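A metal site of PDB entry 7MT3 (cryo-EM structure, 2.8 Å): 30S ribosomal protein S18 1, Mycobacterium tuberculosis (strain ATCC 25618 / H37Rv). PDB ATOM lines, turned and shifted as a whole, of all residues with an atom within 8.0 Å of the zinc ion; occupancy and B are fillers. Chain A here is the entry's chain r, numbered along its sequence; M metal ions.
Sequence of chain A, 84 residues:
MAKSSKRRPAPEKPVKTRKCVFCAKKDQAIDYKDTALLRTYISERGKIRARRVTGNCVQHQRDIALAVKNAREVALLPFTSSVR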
ATOM      1  N   LYS A  19      17.737 -11.816 -20.903  1.00  0.00           N
ATOM      2  CA  LYS A  19      17.836 -11.627 -22.339  1.00  0.00           C
ATOM      3  C   LYS A  19      18.901 -10.575 -22.611  1.00  0.00           C
ATOM      4  O   LYS A  19      19.435 -10.469 -23.706  1.00  0.00           O
ATOM      5  CB  LYS A  19      16.479 -11.242 -22.928  1.00  0.00           C
ATOM      6  CG  LYS A  19      16.313 -11.431 -24.433  1.00  0.00           C
ATOM      7  CD  LYS A  19      16.542 -10.162 -25.219  1.00  0.00           C
ATOM      8  CE  LYS A  19      16.133 -10.344 -26.677  1.00  0.00           C
ATOM      9  NZ  LYS A  19      16.989 -11.340 -27.368  1.00  0.00           N
ATOM     10  N   CYS A  20      19.220  -9.795 -21.569  1.00  0.00           N
ATOM     11  CA  CYS A  20      20.368  -8.914 -21.583  1.00  0.00           C
ATOM     12  C   CYS A  20      21.629  -9.694 -21.240  1.00  0.00           C
ATOM     13  O   CYS A  20      21.566 -10.807 -20.702  1.00  0.00           O
ATOM     14  CB  CYS A  20      20.180  -7.767 -20.603  1.00  0.00           C
ATOM     15  SG  CYS A  20      21.551  -6.603 -20.545  1.00  0.00           S
ATOM     16  N   VAL A  21      22.777  -9.118 -21.545  1.00  0.00           N
ATOM     17  CA  VAL A  21      24.057  -9.795 -21.406  1.00  0.00           C
ATOM     18  C   VAL A  21      24.855  -9.251 -20.219  1.00  0.00           C
ATOM     19  O   VAL A  21      25.476 -10.018 -19.486  1.00  0.00           O
ATOM     20  CB  VAL A  21      24.867  -9.706 -22.710  1.00  0.00           C
ATOM     21  CG1 VAL A  21      26.207 -10.403 -22.598  1.00  0.00           C
ATOM     22  CG2 VAL A  21      24.069 -10.304 -23.860  1.00  0.00           C
ATOM     23  N   PHE A  22      24.805  -7.951 -19.992  1.00  0.00           N
ATOM     24  CA  PHE A  22      25.592  -7.354 -18.925  1.00  0.00           C
ATOM     25  C   PHE A  22      24.877  -7.356 -17.592  1.00  0.00           C
ATOM     26  O   PHE A  22      25.527  -7.200 -16.557  1.00  0.00           O
ATOM     27  CB  PHE A  22      25.970  -5.920 -19.291  1.00  0.00           C
ATOM     28  CG  PHE A  22      26.892  -5.841 -20.455  1.00  0.00           C
ATOM     29  CD1 PHE A  22      28.251  -6.061 -20.288  1.00  0.00           C
ATOM     30  CD2 PHE A  22      26.408  -5.581 -21.722  1.00  0.00           C
ATOM     31  CE1 PHE A  22      29.105  -6.002 -21.368  1.00  0.00           C
ATOM     32  CE2 PHE A  22      27.254  -5.520 -22.791  1.00  0.00           C
ATOM     33  CZ  PHE A  22      28.602  -5.731 -22.614  1.00  0.00           C
ATOM     34  N   CYS A  23      23.557  -7.525 -17.565  1.00  0.00           N
ATOM     35  CA  CYS A  23      22.852  -7.659 -16.301  1.00  0.00           C
ATOM     36  C   CYS A  23      22.906  -9.069 -15.762  1.00  0.00           C
ATOM     37  O   CYS A  23      22.760  -9.274 -14.556  1.00  0.00           O
ATOM     38  CB  CYS A  23      21.397  -7.203 -16.445  1.00  0.00           C
ATOM     39  SG  CYS A  23      21.170  -5.444 -16.756  1.00  0.00           S
ATOM     40  N   ALA A  24      23.103 -10.068 -16.629  1.00  0.00           N
ATOM     41  CA  ALA A  24      23.191 -11.446 -16.170  1.00  0.00           C
ATOM     42  C   ALA A  24      24.517 -11.694 -15.467  1.00  0.00           C
ATOM     43  O   ALA A  24      24.565 -11.962 -14.259  1.00  0.00           O
ATOM     44  CB  ALA A  24      23.007 -12.409 -17.333  1.00  0.00           C
ATOM     45  N   ILE A  30      32.669  -2.511 -18.426  1.00  0.00           N
ATOM     46  CA  ILE A  30      32.583  -1.908 -19.748  1.00  0.00           C
ATOM     47  C   ILE A  30      33.510  -0.697 -19.732  1.00  0.00           C
ATOM     48  O   ILE A  30      33.259   0.272 -19.015  1.00  0.00           O
ATOM     49  CB  ILE A  30      31.157  -1.507 -20.105  1.00  0.00           C
ATOM     50  CG1 ILE A  30      30.283  -2.748 -20.261  1.00  0.00           C
ATOM     51  CG2 ILE A  30      31.136  -0.702 -21.372  1.00  0.00           C
ATOM     52  CD1 ILE A  30      28.829  -2.442 -20.360  1.00  0.00           C
ATOM     53  N   ARG A  51      19.481  -0.870 -29.957  1.00  0.00           N
ATOM     54  CA  ARG A  51      19.208  -1.520 -28.677  1.00  0.00           C
ATOM     55  C   ARG A  51      18.347  -2.753 -28.859  1.00  0.00           C
ATOM     56  O   ARG A  51      18.518  -3.730 -28.123  1.00  0.00           O
ATOM     57  CB  ARG A  51      18.563  -0.497 -27.729  1.00  0.00           C
ATOM     58  CG  ARG A  51      18.218  -0.966 -26.329  1.00  0.00           C
ATOM     59  CD  ARG A  51      16.733  -1.248 -26.225  1.00  0.00           C
ATOM     60  NE  ARG A  51      16.300  -1.562 -24.876  1.00  0.00           N
ATOM     61  CZ  ARG A  51      15.840  -0.654 -24.037  1.00  0.00           C
ATOM     62  NH1 ARG A  51      15.759   0.611 -24.399  1.00  0.00           N
ATOM     63  NH2 ARG A  51      15.446  -1.023 -22.827  1.00  0.00           N
ATOM     64  N   GLY A  55      19.661  -6.473 -27.295  1.00  0.00           N
ATOM     65  CA  GLY A  55      19.002  -6.857 -26.061  1.00  0.00           C
ATOM     66  C   GLY A  55      19.497  -6.159 -24.817  1.00  0.00           C
ATOM     67  O   GLY A  55      19.149  -6.585 -23.717  1.00  0.00           O
ATOM     68  N   ASN A  56      20.288  -5.100 -24.962  1.00  0.00           N
ATOM     69  CA  ASN A  56      20.802  -4.396 -23.798  1.00  0.00           C
ATOM     70  C   ASN A  56      19.693  -3.612 -23.121  1.00  0.00           C
ATOM     71  O   ASN A  56      18.664  -3.286 -23.715  1.00  0.00           O
ATOM     72  CB  ASN A  56      21.917  -3.450 -24.208  1.00  0.00           C
ATOM     73  CG  ASN A  56      23.171  -4.167 -24.604  1.00  0.00           C
ATOM     74  OD1 ASN A  56      23.568  -5.138 -23.967  1.00  0.00           O
ATOM     75  ND2 ASN A  56      23.809  -3.715 -25.663  1.00  0.00           N
ATOM     76  N   CYS A  57      19.906  -3.297 -21.855  1.00  0.00           N
ATOM     77  CA  CYS A  57      19.000  -2.426 -21.139  1.00  0.00           C
ATOM     78  C   CYS A  57      19.302  -0.981 -21.504  1.00  0.00           C
ATOM     79  O   CYS A  57      20.175  -0.693 -22.327  1.00  0.00           O
ATOM     80  CB  CYS A  57      19.090  -2.674 -19.637  1.00  0.00           C
ATOM     81  SG  CYS A  57      20.657  -2.242 -18.867  1.00  0.00           S
ATOM     82  N   VAL A  58      18.563  -0.048 -20.903  1.00  0.00           N
ATOM     83  CA  VAL A  58      18.829   1.362 -21.154  1.00  0.00           C
ATOM     84  C   VAL A  58      20.160   1.777 -20.534  1.00  0.00           C
ATOM     85  O   VAL A  58      20.941   2.507 -21.142  1.00  0.00           O
ATOM     86  CB  VAL A  58      17.666   2.224 -20.618  1.00  0.00           C
ATOM     87  CG1 VAL A  58      17.943   3.693 -20.815  1.00  0.00           C
ATOM     88  CG2 VAL A  58      16.411   1.855 -21.310  1.00  0.00           C
ATOM     89  N   GLN A  59      20.456   1.264 -19.345  1.00  0.00           N
ATOM     90  CA  GLN A  59      21.637   1.717 -18.621  1.00  0.00           C
ATOM     91  C   GLN A  59      22.927   1.131 -19.171  1.00  0.00           C
ATOM     92  O   GLN A  59      23.996   1.697 -18.904  1.00  0.00           O
ATOM     93  CB  GLN A  59      21.510   1.358 -17.150  1.00  0.00           C
ATOM     94  CG  GLN A  59      20.356   2.013 -16.468  1.00  0.00           C
ATOM     95  CD  GLN A  59      20.266   1.647 -15.022  1.00  0.00           C
ATOM     96  OE1 GLN A  59      21.098   0.906 -14.509  1.00  0.00           O
ATOM     97  NE2 GLN A  59      19.241   2.134 -14.348  1.00  0.00           N
ATOM     98  N   HIS A  60      22.863   0.039 -19.904  1.00  0.00           N
ATOM     99  CA  HIS A  60      24.059  -0.536 -20.480  1.00  0.00           C
ATOM    100  C   HIS A  60      24.227  -0.233 -21.964  1.00  0.00           C
ATOM    101  O   HIS A  60      25.362  -0.271 -22.456  1.00  0.00           O
ATOM    102  CB  HIS A  60      24.092  -2.053 -20.266  1.00  0.00           C
ATOM    103  CG  HIS A  60      24.277  -2.442 -18.837  1.00  0.00           C
ATOM    104  ND1 HIS A  60      23.227  -2.696 -17.978  1.00  0.00           N
ATOM    105  CD2 HIS A  60      25.405  -2.609 -18.098  1.00  0.00           C
ATOM    106  CE1 HIS A  60      23.702  -3.009 -16.789  1.00  0.00           C
ATOM    107  NE2 HIS A  60      25.019  -2.952 -16.835  1.00  0.00           N
ATOM    108  N   GLN A  61      23.149   0.071 -22.680  1.00  0.00           N
ATOM    109  CA  GLN A  61      23.300   0.642 -24.008  1.00  0.00           C
ATOM    110  C   GLN A  61      23.888   2.041 -23.927  1.00  0.00           C
ATOM    111  O   GLN A  61      24.655   2.443 -24.817  1.00  0.00           O
ATOM    112  CB  GLN A  61      21.950   0.659 -24.711  1.00  0.00           C
ATOM    113  CG  GLN A  61      21.962   1.182 -26.124  1.00  0.00           C
ATOM    114  CD  GLN A  61      22.738   0.307 -27.058  1.00  0.00           C
ATOM    115  OE1 GLN A  61      22.653  -0.909 -27.007  1.00  0.00           O
ATOM    116  NE2 GLN A  61      23.500   0.930 -27.949  1.00  0.00           N
HETATM  117 ZN    ZN M   1      21.417  -4.566 -19.077  1.00  0.00          ZN
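Within 4 Å of the zinc ion: Cys 20, Cys 23, Cys 57 and His 60.
SG of Cys 23 sits close to ND1 of His 60 (3.6 Å). N of Phe 22 sits close to SG of Cys 20 (3.6 Å). The side-chain sulfur (SG) of Cys 57 lies close to a ring nitrogen (ND1) of His 60 (2.8 Å). N of Gln 59 sits close to SG of Cys 57 (3.5 Å).
The zinc ion is bound by SG of Cys 57 (2.5 Å), SG of Cys 23 (2.5 Å) and SG of Cys 20 (2.5 Å). Slightly farther from the zinc ion lies ND1 of His 60 (2.8 Å).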
